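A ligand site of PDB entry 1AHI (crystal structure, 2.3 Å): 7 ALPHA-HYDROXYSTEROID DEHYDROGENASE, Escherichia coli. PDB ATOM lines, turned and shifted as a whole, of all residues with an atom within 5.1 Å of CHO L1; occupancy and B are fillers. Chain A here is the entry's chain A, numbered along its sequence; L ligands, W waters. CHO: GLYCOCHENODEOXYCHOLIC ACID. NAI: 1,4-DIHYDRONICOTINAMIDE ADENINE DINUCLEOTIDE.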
ATOM      1  N   GLY A  97       2.025  28.163   1.545  1.00  0.00           N
ATOM      2  CA  GLY A  97       1.937  27.146   2.585  1.00  0.00           C
ATOM      3  C   GLY A  97       3.352  26.701   2.870  1.00  0.00           C
ATOM      4  O   GLY A  97       4.267  27.525   2.834  1.00  0.00           O
ATOM      5  N   GLY A  98       3.525  25.421   3.183  1.00  0.00           N
ATOM      6  CA  GLY A  98       4.846  24.903   3.446  1.00  0.00           C
ATOM      7  C   GLY A  98       5.033  24.106   4.730  1.00  0.00           C
ATOM      8  O   GLY A  98       4.087  23.470   5.236  1.00  0.00           O
ATOM      9  N   GLY A  99       6.266  24.118   5.235  1.00  0.00           N
ATOM     10  CA  GLY A  99       6.585  23.381   6.438  1.00  0.00           C
ATOM     11  C   GLY A  99       7.675  22.349   6.196  1.00  0.00           C
ATOM     12  O   GLY A  99       8.755  22.439   6.773  1.00  0.00           O
ATOM     13  N   GLY A 100       7.380  21.334   5.392  1.00  0.00           N
ATOM     14  CA  GLY A 100       8.378  20.325   5.105  1.00  0.00           C
ATOM     15  C   GLY A 100       8.655  19.254   6.150  1.00  0.00           C
ATOM     16  O   GLY A 100       8.076  19.208   7.241  1.00  0.00           O
ATOM     17  N   PRO A 101       9.573  18.352   5.809  1.00  0.00           N
ATOM     18  CA  PRO A 101      10.004  17.234   6.634  1.00  0.00           C
ATOM     19  C   PRO A 101      10.507  17.669   7.998  1.00  0.00           C
ATOM     20  O   PRO A 101      11.357  18.554   8.092  1.00  0.00           O
ATOM     21  CB  PRO A 101      11.149  16.627   5.820  1.00  0.00           C
ATOM     22  CG  PRO A 101      10.793  16.967   4.409  1.00  0.00           C
ATOM     23  CD  PRO A 101      10.334  18.398   4.551  1.00  0.00           C
ATOM     24  N   SER A 146      -1.490  18.961  -0.944  1.00  0.00           N
ATOM     25  CA  SER A 146      -0.333  18.141  -1.256  1.00  0.00           C
ATOM     26  C   SER A 146      -0.699  16.680  -1.188  1.00  0.00           C
ATOM     27  O   SER A 146      -1.710  16.310  -0.586  1.00  0.00           O
ATOM     28  CB  SER A 146       0.823  18.424  -0.285  1.00  0.00           C
ATOM     29  OG  SER A 146       1.867  17.485  -0.452  1.00  0.00           O
ATOM     30  N   MET A 147       0.124  15.852  -1.822  1.00  0.00           N
ATOM     31  CA  MET A 147      -0.075  14.408  -1.830  1.00  0.00           C
ATOM     32  C   MET A 147       0.331  13.825  -0.476  1.00  0.00           C
ATOM     33  O   MET A 147       0.038  12.673  -0.166  1.00  0.00           O
ATOM     34  CB  MET A 147       0.759  13.766  -2.924  1.00  0.00           C
ATOM     35  CG  MET A 147       0.275  14.045  -4.308  1.00  0.00           C
ATOM     36  SD  MET A 147       1.179  12.984  -5.440  1.00  0.00           S
ATOM     37  CE  MET A 147       0.548  11.317  -4.941  1.00  0.00           C
ATOM     38  N   ALA A 148       1.033  14.614   0.310  1.00  0.00           N
ATOM     39  CA  ALA A 148       1.442  14.190   1.638  1.00  0.00           C
ATOM     40  C   ALA A 148       0.170  13.952   2.456  1.00  0.00           C
ATOM     41  O   ALA A 148       0.173  13.186   3.424  1.00  0.00           O
ATOM     42  CB  ALA A 148       2.293  15.279   2.275  1.00  0.00           C
ATOM     43  N   ASN A 151      -0.264  10.382   1.442  1.00  0.00           N
ATOM     44  CA  ASN A 151       0.874   9.516   1.727  1.00  0.00           C
ATOM     45  C   ASN A 151       1.154   9.360   3.213  1.00  0.00           C
ATOM     46  O   ASN A 151       0.811  10.218   4.042  1.00  0.00           O
ATOM     47  CB  ASN A 151       2.147  10.075   1.099  1.00  0.00           C
ATOM     48  CG  ASN A 151       2.021  10.296  -0.312  1.00  0.00           C
ATOM     49  OD1 ASN A 151       1.374   9.522  -1.015  1.00  0.00           O
ATOM     50  ND2 ASN A 151       2.620  11.372  -0.783  1.00  0.00           N
ATOM     51  N   MET A 156       7.257  13.169   8.422  1.00  0.00           N
ATOM     52  CA  MET A 156       6.218  13.980   7.783  1.00  0.00           C
ATOM     53  C   MET A 156       5.058  14.297   8.733  1.00  0.00           C
ATOM     54  O   MET A 156       4.017  14.768   8.288  1.00  0.00           O
ATOM     55  CB  MET A 156       5.652  13.238   6.556  1.00  0.00           C
ATOM     56  CG  MET A 156       6.621  12.993   5.397  1.00  0.00           C
ATOM     57  SD  MET A 156       7.294  14.511   4.640  1.00  0.00           S
ATOM     58  CE  MET A 156       5.788  15.310   4.208  1.00  0.00           C
ATOM     59  N   TYR A 159       3.844  18.266   8.342  1.00  0.00           N
ATOM     60  CA  TYR A 159       3.463  18.585   6.979  1.00  0.00           C
ATOM     61  C   TYR A 159       2.246  17.793   6.535  1.00  0.00           C
ATOM     62  O   TYR A 159       1.217  18.359   6.148  1.00  0.00           O
ATOM     63  CB  TYR A 159       4.627  18.321   6.024  1.00  0.00           C
ATOM     64  CG  TYR A 159       4.398  18.902   4.627  1.00  0.00           C
ATOM     65  CD1 TYR A 159       4.160  20.260   4.460  1.00  0.00           C
ATOM     66  CD2 TYR A 159       4.418  18.093   3.503  1.00  0.00           C
ATOM     67  CE1 TYR A 159       3.947  20.795   3.217  1.00  0.00           C
ATOM     68  CE2 TYR A 159       4.211  18.620   2.256  1.00  0.00           C
ATOM     69  CZ  TYR A 159       3.980  19.983   2.121  1.00  0.00           C
ATOM     70  OH  TYR A 159       3.799  20.525   0.875  1.00  0.00           O
ATOM     71  N   PRO A 189      -0.559  18.465  -5.752  1.00  0.00           N
ATOM     72  CA  PRO A 189       0.567  18.138  -6.628  1.00  0.00           C
ATOM     73  C   PRO A 189       1.615  17.162  -6.092  1.00  0.00           C
ATOM     74  O   PRO A 189       1.761  16.986  -4.870  1.00  0.00           O
ATOM     75  CB  PRO A 189       1.181  19.514  -6.928  1.00  0.00           C
ATOM     76  CG  PRO A 189       0.812  20.342  -5.757  1.00  0.00           C
ATOM     77  CD  PRO A 189      -0.534  19.866  -5.306  1.00  0.00           C
ATOM     78  N   GLY A 190       2.299  16.504  -7.016  1.00  0.00           N
ATOM     79  CA  GLY A 190       3.333  15.551  -6.661  1.00  0.00           C
ATOM     80  C   GLY A 190       4.658  16.289  -6.759  1.00  0.00           C
ATOM     81  O   GLY A 190       4.708  17.487  -6.524  1.00  0.00           O
ATOM     82  N   ALA A 191       5.709  15.584  -7.162  1.00  0.00           N
ATOM     83  CA  ALA A 191       7.023  16.221  -7.267  1.00  0.00           C
ATOM     84  C   ALA A 191       7.064  17.284  -8.341  1.00  0.00           C
ATOM     85  O   ALA A 191       7.320  16.995  -9.505  1.00  0.00           O
ATOM     86  CB  ALA A 191       8.117  15.184  -7.522  1.00  0.00           C
ATOM     87  N   ALA A 196      11.736  24.841  -4.174  1.00  0.00           N
ATOM     88  CA  ALA A 196      11.242  24.193  -2.967  1.00  0.00           C
ATOM     89  C   ALA A 196      11.526  22.699  -3.056  1.00  0.00           C
ATOM     90  O   ALA A 196      11.985  22.085  -2.094  1.00  0.00           O
ATOM     91  CB  ALA A 196       9.747  24.430  -2.812  1.00  0.00           C
ATOM     92  N   LEU A 197      11.274  22.109  -4.221  1.00  0.00           N
ATOM     93  CA  LEU A 197      11.554  20.692  -4.392  1.00  0.00           C
ATOM     94  C   LEU A 197      13.066  20.471  -4.398  1.00  0.00           C
ATOM     95  O   LEU A 197      13.570  19.582  -3.712  1.00  0.00           O
ATOM     96  CB  LEU A 197      10.934  20.151  -5.689  1.00  0.00           C
ATOM     97  CG  LEU A 197      11.072  18.644  -5.912  1.00  0.00           C
ATOM     98  CD1 LEU A 197      10.288  17.871  -4.836  1.00  0.00           C
ATOM     99  CD2 LEU A 197      10.599  18.262  -7.306  1.00  0.00           C
ATOM    100  N   SER A 199      15.453  21.972  -2.888  1.00  0.00           N
ATOM    101  CA  SER A 199      16.085  22.068  -1.587  1.00  0.00           C
ATOM    102  C   SER A 199      16.060  20.765  -0.797  1.00  0.00           C
ATOM    103  O   SER A 199      16.954  20.513   0.013  1.00  0.00           O
ATOM    104  CB  SER A 199      15.450  23.193  -0.760  1.00  0.00           C
ATOM    105  OG  SER A 199      14.252  22.765  -0.133  1.00  0.00           O
ATOM    106  N   VAL A 200      15.036  19.937  -1.032  1.00  0.00           N
ATOM    107  CA  VAL A 200      14.907  18.680  -0.301  1.00  0.00           C
ATOM    108  C   VAL A 200      15.081  17.414  -1.159  1.00  0.00           C
ATOM    109  O   VAL A 200      14.962  16.284  -0.664  1.00  0.00           O
ATOM    110  CB  VAL A 200      13.542  18.610   0.441  1.00  0.00           C
ATOM    111  CG1 VAL A 200      12.424  18.137  -0.486  1.00  0.00           C
ATOM    112  CG2 VAL A 200      13.651  17.713   1.673  1.00  0.00           C
ATOM    113  N   MET A 209      11.789   8.502  -7.387  1.00  0.00           N
ATOM    114  CA  MET A 209      10.540   9.184  -7.714  1.00  0.00           C
ATOM    115  C   MET A 209      10.106   8.835  -9.134  1.00  0.00           C
ATOM    116  O   MET A 209       9.024   8.266  -9.338  1.00  0.00           O
ATOM    117  CB  MET A 209      10.699  10.706  -7.583  1.00  0.00           C
ATOM    118  CG  MET A 209      10.982  11.195  -6.158  1.00  0.00           C
ATOM    119  SD  MET A 209      11.100  13.010  -6.029  1.00  0.00           S
ATOM    120  CE  MET A 209      10.229  13.326  -4.472  1.00  0.00           C
ATOM    121  N   GLN A 252       5.633  10.143  -5.404  1.00  0.00           N
ATOM    122  CA  GLN A 252       6.963  10.688  -5.267  1.00  0.00           C
ATOM    123  C   GLN A 252       7.192  11.067  -3.794  1.00  0.00           C
ATOM    124  O   GLN A 252       6.540  11.991  -3.278  1.00  0.00           O
ATOM    125  CB  GLN A 252       7.133  11.912  -6.170  1.00  0.00           C
ATOM    126  CG  GLN A 252       7.051  11.623  -7.685  1.00  0.00           C
ATOM    127  CD  GLN A 252       5.731  12.098  -8.328  1.00  0.00           C
ATOM    128  OE1 GLN A 252       4.960  12.860  -7.731  1.00  0.00           O
ATOM    129  NE2 GLN A 252       5.484  11.666  -9.552  1.00  0.00           N
ATOM    130  N   GLU A 253       8.067  10.320  -3.129  1.00  0.00           N
ATOM    131  CA  GLU A 253       8.380  10.578  -1.723  1.00  0.00           C
ATOM    132  C   GLU A 253       9.883  10.655  -1.524  1.00  0.00           C
ATOM    133  O   GLU A 253      10.651  10.206  -2.385  1.00  0.00           O
ATOM    134  CB  GLU A 253       7.794   9.477  -0.830  1.00  0.00           C
ATOM    135  CG  GLU A 253       6.288   9.484  -0.795  1.00  0.00           C
ATOM    136  CD  GLU A 253       5.714   8.314  -0.028  1.00  0.00           C
ATOM    137  OE1 GLU A 253       5.745   7.185  -0.557  1.00  0.00           O
ATOM    138  OE2 GLU A 253       5.213   8.531   1.100  1.00  0.00           O
ATOM    139  N   LEU A 254      10.270  11.213  -0.384  1.00  0.00           N
ATOM    140  CA  LEU A 254      11.669  11.393  -0.005  1.00  0.00           C
ATOM    141  C   LEU A 254      12.257  10.229   0.767  1.00  0.00           C
ATOM    142  O   LEU A 254      13.427   9.857   0.587  1.00  0.00           O
ATOM    143  CB  LEU A 254      11.794  12.637   0.865  1.00  0.00           C
ATOM    144  CG  LEU A 254      11.089  13.897   0.375  1.00  0.00           C
ATOM    145  CD1 LEU A 254      10.948  14.892   1.527  1.00  0.00           C
ATOM    146  CD2 LEU A 254      11.851  14.477  -0.808  1.00  0.00           C
HETATM  147  C1  CHO L   1       7.532  14.394  -1.131  1.00  0.00           C
HETATM  148  C2  CHO L   1       6.691  13.892   0.042  1.00  0.00           C
HETATM  149  C3  CHO L   1       5.292  13.584  -0.458  1.00  0.00           C
HETATM  150  O3  CHO L   1       4.464  12.977   0.526  1.00  0.00           O
HETATM  151  C4  CHO L   1       4.664  14.870  -0.959  1.00  0.00           C
HETATM  152  C5  CHO L   1       5.490  15.557  -2.097  1.00  0.00           C
HETATM  153  C6  CHO L   1       4.843  16.869  -2.504  1.00  0.00           C
HETATM  154  C7  CHO L   1       5.115  18.027  -1.529  1.00  0.00           C
HETATM  155  O7  CHO L   1       4.239  18.628  -0.925  1.00  0.00           O
HETATM  156  C8  CHO L   1       6.607  18.284  -1.338  1.00  0.00           C
HETATM  157  C9  CHO L   1       7.253  16.962  -0.807  1.00  0.00           C
HETATM  158  C10 CHO L   1       7.021  15.713  -1.772  1.00  0.00           C
HETATM  159  C11 CHO L   1       8.704  17.188  -0.400  1.00  0.00           C
HETATM  160  C12 CHO L   1       8.903  18.374   0.581  1.00  0.00           C
HETATM  161  C13 CHO L   1       8.440  19.686  -0.025  1.00  0.00           C
HETATM  162  C14 CHO L   1       6.929  19.497  -0.362  1.00  0.00           C
HETATM  163  C15 CHO L   1       6.505  20.919  -0.741  1.00  0.00           C
HETATM  164  C16 CHO L   1       7.186  21.732   0.379  1.00  0.00           C
HETATM  165  C17 CHO L   1       8.350  20.914   0.938  1.00  0.00           C
HETATM  166  C18 CHO L   1       9.297  20.086  -1.263  1.00  0.00           C
HETATM  167  C19 CHO L   1       7.833  15.835  -3.056  1.00  0.00           C
HETATM  168  C20 CHO L   1       9.607  21.771   1.240  1.00  0.00           C
HETATM  169  C21 CHO L   1      10.786  20.945   1.816  1.00  0.00           C
HETATM  170  C22 CHO L   1       9.162  22.808   2.250  1.00  0.00           C
HETATM  171  C23 CHO L   1      10.249  23.785   2.712  1.00  0.00           C
HETATM  172  C24 CHO L   1       9.698  24.843   3.761  1.00  0.00           C
HETATM  173  O24 CHO L   1       8.656  25.480   3.491  1.00  0.00           O
HETATM  174  N25 CHO L   1      10.336  25.010   4.841  1.00  0.00           N
HETATM  175  PA  NAI L   2       8.082  27.999  -3.408  1.00  0.00           P
HETATM  176  O1A NAI L   2       8.637  28.019  -2.027  1.00  0.00           O
HETATM  177  O2A NAI L   2       9.000  27.721  -4.560  1.00  0.00           O
HETATM  178  O5B NAI L   2       7.368  29.417  -3.713  1.00  0.00           O
HETATM  179  C5B NAI L   2       6.360  29.900  -2.836  1.00  0.00           C
HETATM  180  C4B NAI L   2       6.247  31.418  -2.770  1.00  0.00           C
HETATM  181  O4B NAI L   2       5.563  31.598  -1.505  1.00  0.00           O
HETATM  182  C3B NAI L   2       7.588  32.125  -2.627  1.00  0.00           C
HETATM  183  O3B NAI L   2       7.747  33.266  -3.522  1.00  0.00           O
HETATM  184  C2B NAI L   2       7.627  32.556  -1.170  1.00  0.00           C
HETATM  185  O2B NAI L   2       8.256  33.831  -1.134  1.00  0.00           O
HETATM  186  C1B NAI L   2       6.161  32.679  -0.789  1.00  0.00           C
HETATM  187  N9A NAI L   2       5.818  32.629   0.662  1.00  0.00           N
HETATM  188  C8A NAI L   2       6.348  31.773   1.565  1.00  0.00           C
HETATM  189  N7A NAI L   2       5.822  31.963   2.793  1.00  0.00           N
HETATM  190  C5A NAI L   2       4.958  32.966   2.613  1.00  0.00           C
HETATM  191  C6A NAI L   2       4.167  33.521   3.612  1.00  0.00           C
HETATM  192  N6A NAI L   2       4.308  33.069   4.847  1.00  0.00           N
HETATM  193  N1A NAI L   2       3.331  34.530   3.262  1.00  0.00           N
HETATM  194  C2A NAI L   2       3.283  34.962   2.000  1.00  0.00           C
HETATM  195  N3A NAI L   2       4.056  34.416   1.047  1.00  0.00           N
HETATM  196  C4A NAI L   2       4.924  33.398   1.307  1.00  0.00           C
HETATM  197  O3  NAI L   2       6.851  26.966  -3.418  1.00  0.00           O
HETATM  198  PN  NAI L   2       6.070  26.147  -4.550  1.00  0.00           P
HETATM  199  O1N NAI L   2       6.946  24.976  -4.893  1.00  0.00           O
HETATM  200  O2N NAI L   2       5.630  27.102  -5.612  1.00  0.00           O
HETATM  201  O5D NAI L   2       4.789  25.506  -3.777  1.00  0.00           O
HETATM  202  C5D NAI L   2       3.837  26.263  -2.993  1.00  0.00           C
HETATM  203  C4D NAI L   2       2.677  25.395  -2.470  1.00  0.00           C
HETATM  204  O4D NAI L   2       2.630  24.162  -3.209  1.00  0.00           O
HETATM  205  C3D NAI L   2       2.809  24.997  -0.997  1.00  0.00           C
HETATM  206  O3D NAI L   2       1.520  25.021  -0.288  1.00  0.00           O
HETATM  207  C2D NAI L   2       3.356  23.561  -1.015  1.00  0.00           C
HETATM  208  O2D NAI L   2       2.922  22.907   0.204  1.00  0.00           O
HETATM  209  C1D NAI L   2       2.678  23.060  -2.283  1.00  0.00           C
HETATM  210  N1N NAI L   2       3.334  21.924  -2.979  1.00  0.00           N
HETATM  211  C2N NAI L   2       4.574  22.026  -3.677  1.00  0.00           C
HETATM  212  C3N NAI L   2       5.104  20.930  -4.389  1.00  0.00           C
HETATM  213  C7N NAI L   2       6.491  20.913  -5.055  1.00  0.00           C
HETATM  214  O7N NAI L   2       6.974  19.817  -5.341  1.00  0.00           O
HETATM  215  N7N NAI L   2       7.135  22.067  -5.266  1.00  0.00           N
HETATM  216  C4N NAI L   2       4.390  19.742  -4.399  1.00  0.00           C
HETATM  217  C5N NAI L   2       3.187  19.636  -3.697  1.00  0.00           C
HETATM  218  C6N NAI L   2       2.650  20.702  -2.983  1.00  0.00           C
HETATM  219  O   HOH W   1       8.253  11.482   1.908  1.00  0.00           O
HETATM  220  O   HOH W   2       5.540  11.097   2.153  1.00  0.00           O
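Residues that only touch CHO L1: Gln 252 (3.4 Å), Ala 148 (3.4 Å), Ala 196 (3.5 Å), Leu 197 (3.7 Å), Val 200 (3.7 Å), Leu 254 (3.7 Å), Met 209 (3.7 Å), Pro 101 (3.8 Å), Gly 98 (3.9 Å), Gly 100 (3.9 Å), Pro 189 (3.9 Å) and Glu 253 (3.95 Å). Hydrophobic or aromatic side chains that line CHO L1: Pro 101, Ala 148, Tyr 159, Leu 197, Val 200, Met 209 and Leu 254. Within 4 Å of CHO L1: Gly 98, Gly 99, Gly 100, Pro 101, Ser 146, Ala 148, Asn 151, Tyr 159, Pro 189, Ala 196, Leu 197, Val 200, Met 209, Gln 252, Glu 253 and Leu 254. Along chain A the residues within 4 Å of CHO L1 span positions 98 to 254.
The side-chain amide oxygen of Gln 252 sits at hydrogen-bond distance from the backbone NH of Ala 191, 2.9 Å away. The backbone NH (N) of Ala 148 sits close to the side-chain hydroxyl (OG) of Ser 146, at 3.1 Å. ND2 of Asn 151 lies within hydrogen-bond range of O of Met 147, 3.0 Å away. O of Ala 196 lies within hydrogen-bond range of OG of Ser 199 (3.1 Å).
ND2 of Asn 151 lies within hydrogen-bond range of O3 of CHO L1 (2.8 Å). The side-chain hydroxyl (OH) of Tyr 159 is in hydrogen-bond range of an oxygen (O7) of CHO L1 (2.7 Å). An oxygen (O2D) of NAI L2 is in hydrogen-bond range of the side-chain hydroxyl of Tyr 159. O7 of CHO L1 is in hydrogen-bond range of OG of Ser 146, at 2.7 Å. The backbone NH (N) of Gly 99 lies within hydrogen-bond range of an oxygen (O24) of CHO L1, 3.3 Å away.
Water W2 lies within hydrogen-bond range of an oxygen (O3) of CHO L1 (2.7 Å) and the side-chain carboxylate (OE2) of Glu 253 (2.8 Å).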
